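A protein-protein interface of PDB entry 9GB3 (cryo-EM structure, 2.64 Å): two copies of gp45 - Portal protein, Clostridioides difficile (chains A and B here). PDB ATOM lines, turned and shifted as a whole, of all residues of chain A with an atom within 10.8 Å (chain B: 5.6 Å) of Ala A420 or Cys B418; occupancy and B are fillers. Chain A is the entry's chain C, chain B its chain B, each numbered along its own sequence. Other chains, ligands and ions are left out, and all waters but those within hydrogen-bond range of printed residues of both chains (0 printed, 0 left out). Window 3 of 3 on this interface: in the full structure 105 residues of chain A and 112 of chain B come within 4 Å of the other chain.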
ATOM      1  N   ALA A 411     -14.813   8.168 -21.364  1.00  0.00           N
ATOM      2  CA  ALA A 411     -13.953   7.468 -22.311  1.00  0.00           C
ATOM      3  C   ALA A 411     -12.689   6.949 -21.630  1.00  0.00           C
ATOM      4  O   ALA A 411     -12.159   5.899 -22.009  1.00  0.00           O
ATOM      5  CB  ALA A 411     -13.601   8.390 -23.476  1.00  0.00           C
ATOM      6  N   GLU A 412     -12.190   7.670 -20.625  1.00  0.00           N
ATOM      7  CA  GLU A 412     -11.027   7.196 -19.880  1.00  0.00           C
ATOM      8  C   GLU A 412     -11.339   5.896 -19.149  1.00  0.00           C
ATOM      9  O   GLU A 412     -10.558   4.938 -19.195  1.00  0.00           O
ATOM     10  CB  GLU A 412     -10.570   8.272 -18.895  1.00  0.00           C
ATOM     11  CG  GLU A 412      -9.776   9.395 -19.540  1.00  0.00           C
ATOM     12  CD  GLU A 412      -9.498  10.544 -18.591  1.00  0.00           C
ATOM     13  OE1 GLU A 412     -10.031  10.535 -17.462  1.00  0.00           O
ATOM     14  OE2 GLU A 412      -8.743  11.461 -18.978  1.00  0.00           O
ATOM     15  N   THR A 413     -12.484   5.840 -18.468  1.00  0.00           N
ATOM     16  CA  THR A 413     -12.847   4.595 -17.797  1.00  0.00           C
ATOM     17  C   THR A 413     -13.191   3.503 -18.804  1.00  0.00           C
ATOM     18  O   THR A 413     -12.996   2.317 -18.518  1.00  0.00           O
ATOM     19  CB  THR A 413     -13.993   4.827 -16.803  1.00  0.00           C
ATOM     20  OG1 THR A 413     -14.271   3.615 -16.090  1.00  0.00           O
ATOM     21  CG2 THR A 413     -15.252   5.311 -17.476  1.00  0.00           C
ATOM     22  N   LEU A 414     -13.688   3.875 -19.988  1.00  0.00           N
ATOM     23  CA  LEU A 414     -13.857   2.895 -21.057  1.00  0.00           C
ATOM     24  C   LEU A 414     -12.515   2.287 -21.444  1.00  0.00           C
ATOM     25  O   LEU A 414     -12.405   1.074 -21.649  1.00  0.00           O
ATOM     26  CB  LEU A 414     -14.526   3.549 -22.271  1.00  0.00           C
ATOM     27  CG  LEU A 414     -14.773   2.709 -23.532  1.00  0.00           C
ATOM     28  CD1 LEU A 414     -15.833   1.640 -23.316  1.00  0.00           C
ATOM     29  CD2 LEU A 414     -15.170   3.616 -24.684  1.00  0.00           C
ATOM     30  N   GLU A 415     -11.483   3.124 -21.555  1.00  0.00           N
ATOM     31  CA  GLU A 415     -10.137   2.626 -21.832  1.00  0.00           C
ATOM     32  C   GLU A 415      -9.663   1.695 -20.726  1.00  0.00           C
ATOM     33  O   GLU A 415      -9.066   0.643 -20.992  1.00  0.00           O
ATOM     34  CB  GLU A 415      -9.166   3.796 -21.983  1.00  0.00           C
ATOM     35  CG  GLU A 415      -9.218   4.478 -23.323  1.00  0.00           C
ATOM     36  CD  GLU A 415      -8.612   3.633 -24.418  1.00  0.00           C
ATOM     37  OE1 GLU A 415      -7.564   2.996 -24.183  1.00  0.00           O
ATOM     38  OE2 GLU A 415      -9.200   3.592 -25.510  1.00  0.00           O
ATOM     39  N   LYS A 416      -9.900   2.087 -19.474  1.00  0.00           N
ATOM     40  CA  LYS A 416      -9.475   1.266 -18.344  1.00  0.00           C
ATOM     41  C   LYS A 416     -10.148  -0.102 -18.384  1.00  0.00           C
ATOM     42  O   LYS A 416      -9.497  -1.136 -18.190  1.00  0.00           O
ATOM     43  CB  LYS A 416      -9.783   1.986 -17.032  1.00  0.00           C
ATOM     44  CG  LYS A 416      -8.985   3.271 -16.799  1.00  0.00           C
ATOM     45  CD  LYS A 416      -7.504   3.006 -16.575  1.00  0.00           C
ATOM     46  CE  LYS A 416      -6.672   3.348 -17.802  1.00  0.00           C
ATOM     47  NZ  LYS A 416      -5.218   3.131 -17.564  1.00  0.00           N
ATOM     48  N   VAL A 417     -11.452  -0.127 -18.661  1.00  0.00           N
ATOM     49  CA  VAL A 417     -12.176  -1.393 -18.747  1.00  0.00           C
ATOM     50  C   VAL A 417     -11.663  -2.222 -19.917  1.00  0.00           C
ATOM     51  O   VAL A 417     -11.472  -3.439 -19.802  1.00  0.00           O
ATOM     52  CB  VAL A 417     -13.690  -1.138 -18.863  1.00  0.00           C
ATOM     53  CG1 VAL A 417     -14.432  -2.427 -19.197  1.00  0.00           C
ATOM     54  CG2 VAL A 417     -14.228  -0.542 -17.578  1.00  0.00           C
ATOM     55  N   CYS A 418     -11.447  -1.579 -21.069  1.00  0.00           N
ATOM     56  CA  CYS A 418     -11.040  -2.310 -22.264  1.00  0.00           C
ATOM     57  C   CYS A 418      -9.680  -2.965 -22.072  1.00  0.00           C
ATOM     58  O   CYS A 418      -9.489  -4.137 -22.414  1.00  0.00           O
ATOM     59  CB  CYS A 418     -11.021  -1.369 -23.469  1.00  0.00           C
ATOM     60  SG  CYS A 418     -10.472  -2.149 -25.004  1.00  0.00           S
ATOM     61  N   CYS A 419      -8.717  -2.226 -21.515  1.00  0.00           N
ATOM     62  CA  CYS A 419      -7.412  -2.828 -21.267  1.00  0.00           C
ATOM     63  C   CYS A 419      -7.477  -3.839 -20.131  1.00  0.00           C
ATOM     64  O   CYS A 419      -6.695  -4.797 -20.112  1.00  0.00           O
ATOM     65  CB  CYS A 419      -6.369  -1.752 -20.970  1.00  0.00           C
ATOM     66  SG  CYS A 419      -6.719  -0.753 -19.525  1.00  0.00           S
ATOM     67  N   ALA A 420      -8.392  -3.649 -19.175  1.00  0.00           N
ATOM     68  CA  ALA A 420      -8.615  -4.678 -18.164  1.00  0.00           C
ATOM     69  C   ALA A 420      -9.127  -5.961 -18.803  1.00  0.00           C
ATOM     70  O   ALA A 420      -8.680  -7.060 -18.457  1.00  0.00           O
ATOM     71  CB  ALA A 420      -9.599  -4.175 -17.108  1.00  0.00           C
ATOM     72  N   LEU A 421     -10.061  -5.841 -19.743  1.00  0.00           N
ATOM     73  CA  LEU A 421     -10.525  -6.993 -20.498  1.00  0.00           C
ATOM     74  C   LEU A 421      -9.453  -7.415 -21.501  1.00  0.00           C
ATOM     75  O   LEU A 421      -8.377  -6.816 -21.595  1.00  0.00           O
ATOM     76  CB  LEU A 421     -11.849  -6.672 -21.190  1.00  0.00           C
ATOM     77  CG  LEU A 421     -13.015  -6.332 -20.258  1.00  0.00           C
ATOM     78  CD1 LEU A 421     -14.169  -5.729 -21.042  1.00  0.00           C
ATOM     79  CD2 LEU A 421     -13.476  -7.564 -19.493  1.00  0.00           C
ATOM     80  N   ASP A 422      -9.749  -8.470 -22.256  1.00  0.00           N
ATOM     81  CA  ASP A 422      -8.816  -9.107 -23.183  1.00  0.00           C
ATOM     82  C   ASP A 422      -7.610  -9.714 -22.473  1.00  0.00           C
ATOM     83  O   ASP A 422      -6.582  -9.967 -23.114  1.00  0.00           O
ATOM     84  CB  ASP A 422      -8.337  -8.128 -24.265  1.00  0.00           C
ATOM     85  CG  ASP A 422      -9.475  -7.346 -24.891  1.00  0.00           C
ATOM     86  OD1 ASP A 422     -10.647  -7.706 -24.659  1.00  0.00           O
ATOM     87  OD2 ASP A 422      -9.196  -6.367 -25.614  1.00  0.00           O
ATOM     88  N   LYS A 423      -7.707  -9.949 -21.165  1.00  0.00           N
ATOM     89  CA  LYS A 423      -6.650 -10.571 -20.381  1.00  0.00           C
ATOM     90  C   LYS A 423      -7.300 -11.498 -19.367  1.00  0.00           C
ATOM     91  O   LYS A 423      -8.420 -11.250 -18.912  1.00  0.00           O
ATOM     92  CB  LYS A 423      -5.782  -9.524 -19.672  1.00  0.00           C
ATOM     93  CG  LYS A 423      -5.103  -8.545 -20.613  1.00  0.00           C
ATOM     94  CD  LYS A 423      -4.231  -7.554 -19.861  1.00  0.00           C
ATOM     95  CE  LYS A 423      -3.645  -6.512 -20.799  1.00  0.00           C
ATOM     96  NZ  LYS A 423      -2.719  -5.580 -20.096  1.00  0.00           N
ATOM     97  N   ALA A 424      -6.587 -12.569 -19.012  1.00  0.00           N
ATOM     98  CA  ALA A 424      -7.144 -13.642 -18.188  1.00  0.00           C
ATOM     99  C   ALA A 424      -8.408 -14.200 -18.845  1.00  0.00           C
ATOM    100  O   ALA A 424      -9.522 -14.079 -18.333  1.00  0.00           O
ATOM    101  CB  ALA A 424      -7.421 -13.158 -16.761  1.00  0.00           C
ATOM    102  N   LEU A 425      -8.204 -14.823 -20.007  1.00  0.00           N
ATOM    103  CA  LEU A 425      -9.281 -15.165 -20.934  1.00  0.00           C
ATOM    104  C   LEU A 425     -10.197 -16.283 -20.441  1.00  0.00           C
ATOM    105  O   LEU A 425     -11.077 -16.700 -21.204  1.00  0.00           O
ATOM    106  CB  LEU A 425      -8.682 -15.555 -22.287  1.00  0.00           C
ATOM    107  CG  LEU A 425      -7.708 -14.553 -22.919  1.00  0.00           C
ATOM    108  CD1 LEU A 425      -7.154 -15.103 -24.224  1.00  0.00           C
ATOM    109  CD2 LEU A 425      -8.367 -13.199 -23.142  1.00  0.00           C
ATOM    110  N   GLU A 426     -10.033 -16.782 -19.214  1.00  0.00           N
ATOM    111  CA  GLU A 426     -10.958 -17.766 -18.666  1.00  0.00           C
ATOM    112  C   GLU A 426     -12.316 -17.172 -18.299  1.00  0.00           C
ATOM    113  O   GLU A 426     -13.225 -17.936 -17.956  1.00  0.00           O
ATOM    114  CB  GLU A 426     -10.347 -18.429 -17.428  1.00  0.00           C
ATOM    115  CG  GLU A 426      -8.954 -19.019 -17.634  1.00  0.00           C
ATOM    116  CD  GLU A 426      -8.903 -20.046 -18.748  1.00  0.00           C
ATOM    117  OE1 GLU A 426      -9.895 -20.784 -18.925  1.00  0.00           O
ATOM    118  OE2 GLU A 426      -7.868 -20.119 -19.444  1.00  0.00           O
ATOM    119  N   GLY A 427     -12.482 -15.849 -18.356  1.00  0.00           N
ATOM    120  CA  GLY A 427     -13.716 -15.213 -17.933  1.00  0.00           C
ATOM    121  C   GLY A 427     -14.898 -15.385 -18.862  1.00  0.00           C
ATOM    122  O   GLY A 427     -16.018 -15.034 -18.476  1.00  0.00           O
ATOM    123  N   GLY A 428     -14.686 -15.906 -20.064  1.00  0.00           N
ATOM    124  CA  GLY A 428     -15.775 -16.107 -20.998  1.00  0.00           C
ATOM    125  C   GLY A 428     -16.070 -14.873 -21.824  1.00  0.00           C
ATOM    126  O   GLY A 428     -15.359 -13.862 -21.792  1.00  0.00           O
ATOM    127  N   SER A 431     -17.533 -10.390 -21.561  1.00  0.00           N
ATOM    128  CA  SER A 431     -16.905  -9.114 -21.879  1.00  0.00           C
ATOM    129  C   SER A 431     -17.688  -8.385 -22.961  1.00  0.00           C
ATOM    130  O   SER A 431     -17.811  -7.157 -22.928  1.00  0.00           O
ATOM    131  CB  SER A 431     -15.459  -9.337 -22.323  1.00  0.00           C
ATOM    132  OG  SER A 431     -15.395 -10.259 -23.397  1.00  0.00           O
ATOM    133  N   SER A 434     -20.711  -6.838 -21.226  1.00  0.00           N
ATOM    134  CA  SER A 434     -20.360  -5.633 -20.481  1.00  0.00           C
ATOM    135  C   SER A 434     -20.049  -4.468 -21.415  1.00  0.00           C
ATOM    136  O   SER A 434     -20.537  -3.349 -21.212  1.00  0.00           O
ATOM    137  CB  SER A 434     -19.168  -5.913 -19.565  1.00  0.00           C
ATOM    138  OG  SER A 434     -18.892  -4.801 -18.732  1.00  0.00           O
ATOM    139  N   THR A 435     -19.250  -4.715 -22.456  1.00  0.00           N
ATOM    140  CA  THR A 435     -18.747  -3.617 -23.270  1.00  0.00           C
ATOM    141  C   THR A 435     -19.830  -3.057 -24.186  1.00  0.00           C
ATOM    142  O   THR A 435     -19.839  -1.856 -24.464  1.00  0.00           O
ATOM    143  CB  THR A 435     -17.524  -4.070 -24.075  1.00  0.00           C
ATOM    144  OG1 THR A 435     -16.840  -2.922 -24.595  1.00  0.00           O
ATOM    145  CG2 THR A 435     -17.920  -4.978 -25.228  1.00  0.00           C
ATOM    146  N   ALA B 411     -12.426   1.084 -12.473  1.00  0.00           N
ATOM    147  CA  ALA B 411     -11.753   0.414 -13.581  1.00  0.00           C
ATOM    148  C   ALA B 411     -10.240   0.417 -13.388  1.00  0.00           C
ATOM    149  O   ALA B 411      -9.554  -0.532 -13.791  1.00  0.00           O
ATOM    150  CB  ALA B 411     -12.134   1.079 -14.900  1.00  0.00           C
ATOM    151  N   THR B 413      -8.594   0.241 -10.440  1.00  0.00           N
ATOM    152  CA  THR B 413      -8.263  -0.844  -9.522  1.00  0.00           C
ATOM    153  C   THR B 413      -8.548  -2.204 -10.152  1.00  0.00           C
ATOM    154  O   THR B 413      -7.869  -3.186  -9.835  1.00  0.00           O
ATOM    155  CB  THR B 413      -9.000  -0.666  -8.185  1.00  0.00           C
ATOM    156  OG1 THR B 413      -8.585  -1.680  -7.262  1.00  0.00           O
ATOM    157  CG2 THR B 413     -10.514  -0.700  -8.321  1.00  0.00           C
ATOM    158  N   LEU B 414      -9.519  -2.275 -11.068  1.00  0.00           N
ATOM    159  CA  LEU B 414      -9.768  -3.520 -11.787  1.00  0.00           C
ATOM    160  C   LEU B 414      -8.557  -3.920 -12.621  1.00  0.00           C
ATOM    161  O   LEU B 414      -8.121  -5.075 -12.585  1.00  0.00           O
ATOM    162  CB  LEU B 414     -11.010  -3.372 -12.673  1.00  0.00           C
ATOM    163  CG  LEU B 414     -11.400  -4.513 -13.624  1.00  0.00           C
ATOM    164  CD1 LEU B 414     -11.844  -5.762 -12.877  1.00  0.00           C
ATOM    165  CD2 LEU B 414     -12.502  -4.042 -14.554  1.00  0.00           C
ATOM    166  N   GLU B 415      -7.996  -2.975 -13.381  1.00  0.00           N
ATOM    167  CA  GLU B 415      -6.832  -3.314 -14.195  1.00  0.00           C
ATOM    168  C   GLU B 415      -5.616  -3.596 -13.322  1.00  0.00           C
ATOM    169  O   GLU B 415      -4.771  -4.427 -13.677  1.00  0.00           O
ATOM    170  CB  GLU B 415      -6.522  -2.208 -15.208  1.00  0.00           C
ATOM    171  CG  GLU B 415      -6.168  -0.849 -14.620  1.00  0.00           C
ATOM    172  CD  GLU B 415      -5.549   0.095 -15.632  1.00  0.00           C
ATOM    173  OE1 GLU B 415      -5.395  -0.296 -16.807  1.00  0.00           O
ATOM    174  OE2 GLU B 415      -5.209   1.233 -15.247  1.00  0.00           O
ATOM    175  N   LYS B 416      -5.500  -2.908 -12.183  1.00  0.00           N
ATOM    176  CA  LYS B 416      -4.393  -3.194 -11.277  1.00  0.00           C
ATOM    177  C   LYS B 416      -4.494  -4.612 -10.728  1.00  0.00           C
ATOM    178  O   LYS B 416      -3.489  -5.329 -10.642  1.00  0.00           O
ATOM    179  CB  LYS B 416      -4.355  -2.170 -10.143  1.00  0.00           C
ATOM    180  CG  LYS B 416      -3.989  -0.761 -10.597  1.00  0.00           C
ATOM    181  CD  LYS B 416      -2.513  -0.638 -10.969  1.00  0.00           C
ATOM    182  CE  LYS B 416      -1.759   0.286 -10.030  1.00  0.00           C
ATOM    183  NZ  LYS B 416      -0.424   0.661 -10.573  1.00  0.00           N
ATOM    184  N   VAL B 417      -5.705  -5.043 -10.371  1.00  0.00           N
ATOM    185  CA  VAL B 417      -5.902  -6.419  -9.925  1.00  0.00           C
ATOM    186  C   VAL B 417      -5.598  -7.389 -11.059  1.00  0.00           C
ATOM    187  O   VAL B 417      -4.986  -8.443 -10.848  1.00  0.00           O
ATOM    188  CB  VAL B 417      -7.332  -6.610  -9.388  1.00  0.00           C
ATOM    189  CG1 VAL B 417      -7.639  -8.088  -9.173  1.00  0.00           C
ATOM    190  CG2 VAL B 417      -7.524  -5.840  -8.095  1.00  0.00           C
ATOM    191  N   CYS B 418      -6.030  -7.056 -12.277  1.00  0.00           N
ATOM    192  CA  CYS B 418      -5.822  -7.949 -13.412  1.00  0.00           C
ATOM    193  C   CYS B 418      -4.338  -8.158 -13.686  1.00  0.00           C
ATOM    194  O   CYS B 418      -3.871  -9.297 -13.794  1.00  0.00           O
ATOM    195  CB  CYS B 418      -6.519  -7.391 -14.653  1.00  0.00           C
ATOM    196  SG  CYS B 418      -6.136  -8.291 -16.172  1.00  0.00           S
ATOM    197  N   CYS B 419      -3.576  -7.067 -13.792  1.00  0.00           N
ATOM    198  CA  CYS B 419      -2.150  -7.205 -14.062  1.00  0.00           C
ATOM    199  C   CYS B 419      -1.394  -7.749 -12.856  1.00  0.00           C
ATOM    200  O   CYS B 419      -0.312  -8.320 -13.028  1.00  0.00           O
ATOM    201  CB  CYS B 419      -1.555  -5.867 -14.509  1.00  0.00           C
ATOM    202  SG  CYS B 419      -1.041  -4.766 -13.183  1.00  0.00           S
ATOM    203  N   ALA B 420      -1.933  -7.589 -11.644  1.00  0.00           N
ATOM    204  CA  ALA B 420      -1.387  -8.315 -10.503  1.00  0.00           C
ATOM    205  C   ALA B 420      -1.560  -9.815 -10.689  1.00  0.00           C
ATOM    206  O   ALA B 420      -0.652 -10.598 -10.387  1.00  0.00           O
ATOM    207  CB  ALA B 420      -2.056  -7.851  -9.211  1.00  0.00           C
ATOM    208  N   LEU B 421      -2.720 -10.233 -11.188  1.00  0.00           N
ATOM    209  CA  LEU B 421      -2.946 -11.630 -11.518  1.00  0.00           C
ATOM    210  C   LEU B 421      -2.175 -11.986 -12.789  1.00  0.00           C
ATOM    211  O   LEU B 421      -1.459 -11.163 -13.368  1.00  0.00           O
ATOM    212  CB  LEU B 421      -4.443 -11.897 -11.669  1.00  0.00           C
ATOM    213  CG  LEU B 421      -5.282 -11.642 -10.412  1.00  0.00           C
ATOM    214  CD1 LEU B 421      -6.757 -11.536 -10.764  1.00  0.00           C
ATOM    215  CD2 LEU B 421      -5.050 -12.730  -9.377  1.00  0.00           C
ATOM    216  N   ASP B 422      -2.314 -13.240 -13.223  1.00  0.00           N
ATOM    217  CA  ASP B 422      -1.536 -13.800 -14.328  1.00  0.00           C
ATOM    218  C   ASP B 422      -0.035 -13.761 -14.047  1.00  0.00           C
ATOM    219  O   ASP B 422       0.774 -13.735 -14.980  1.00  0.00           O
ATOM    220  CB  ASP B 422      -1.842 -13.086 -15.651  1.00  0.00           C
ATOM    221  CG  ASP B 422      -3.320 -13.081 -15.984  1.00  0.00           C
ATOM    222  OD1 ASP B 422      -4.043 -13.979 -15.505  1.00  0.00           O
ATOM    223  OD2 ASP B 422      -3.760 -12.178 -16.726  1.00  0.00           O
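SG of Cys B418 lies within hydrogen-bond range of O of Ala A420.
The side-chain carboxylate (OE2) of Glu B415 is in salt-bridge range of the side-chain amino group (NZ) of Lys A416, 3.0 Å away.
The side-chain carboxylate (OE1) of Glu B415 lies within hydrogen-bond range of the side-chain sulfur (SG) of Cys A419 (3.1 Å).
O of Glu A415 sits at hydrogen-bond distance from SG of Cys A419 (3.1 Å).
The backbone carbonyl oxygen (O) of Lys A416 lies within hydrogen-bond range of the side-chain sulfur (SG) of Cys A419, 3.1 Å away.
The side-chain sulfur of Cys B419 lies close to the backbone carbonyl oxygen of Glu B415 (3.8 Å).
Among the printed residues, merely in contact across the chains: Lys A416 with Ala B411, Thr A413 with Ala B411, Ala A424 with Asp B422, Lys A423 with Cys B418, Val A417 with Ala B411 and Ala A420 with Leu B414.
Of the printed residues of chain B, Lys A416 touches Ala B411 and Glu B415.
Printed residues of chain B within 4 Å of Cys A419: Glu B415 (3.1 Å).
Of chain B, only Leu B414 and Cys B418 come within 4 Å of Ala A420.
Printed residues of chain B within 4 Å of Lys A423: Cys B418 (3.7 Å).
Of the printed residues of chain B, Ala A424 touches Asp B422 (3.7 Å).
Ser A434 touches none of the printed residues of chain B.
Of the printed residues of chain A, Ala B411 touches Thr A413 (3.5 Å), Lys A416 (3.3 Å) and Val A417 (3.8 Å).
Leu B414 touches one residue of chain A.
No residue of chain A comes within 4 Å of Val B417.
Of the printed residues of chain A, Cys B418 touches Ala A420 (3.6 Å) and Lys A423 (3.7 Å).
No residue of chain A comes within 4 Å of Ala B420.
No residue of chain A comes within 4 Å of Leu B421.
The nearest residue of chain A that does not touch Cys B418 is Ala A424 (5.1 Å).
The nearest printed residue of chain B that does not touch Cys A419 is Cys B418 (5.3 Å).
Hydrophobic or aromatic side chains of chain B within 4 Å of the printed part of chain A: Ala B411 and Leu B414.
Of the 21 printed residues of chain A, 7 touch a printed residue of chain B.
Among the printed residues, Asp or Glu carboxylates within 4 Å of a Lys or Arg side-chain nitrogen of the other chain: Lys A416 with Glu B415.
Thr A413 touches Ala B411, but with the chains exchanged Ala A411 does not touch Thr B413 (13.4 Å).
Lys A416 touches Ala B411, but with the chains exchanged Ala A411 does not touch Lys B416 (14.8 Å).
Cys A419 touches Glu B415, but with the chains exchanged Glu A415 does not touch Cys B419 (11.9 Å).
Ala A420 touches Cys B418, but with the chains exchanged Cys A418 does not touch Ala B420 (13.6 Å).
11 positions are printed for both chains.
Of the 9 pairs that touch across the chains among the printed residues, none has its exchanged pair printed and touching as well.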
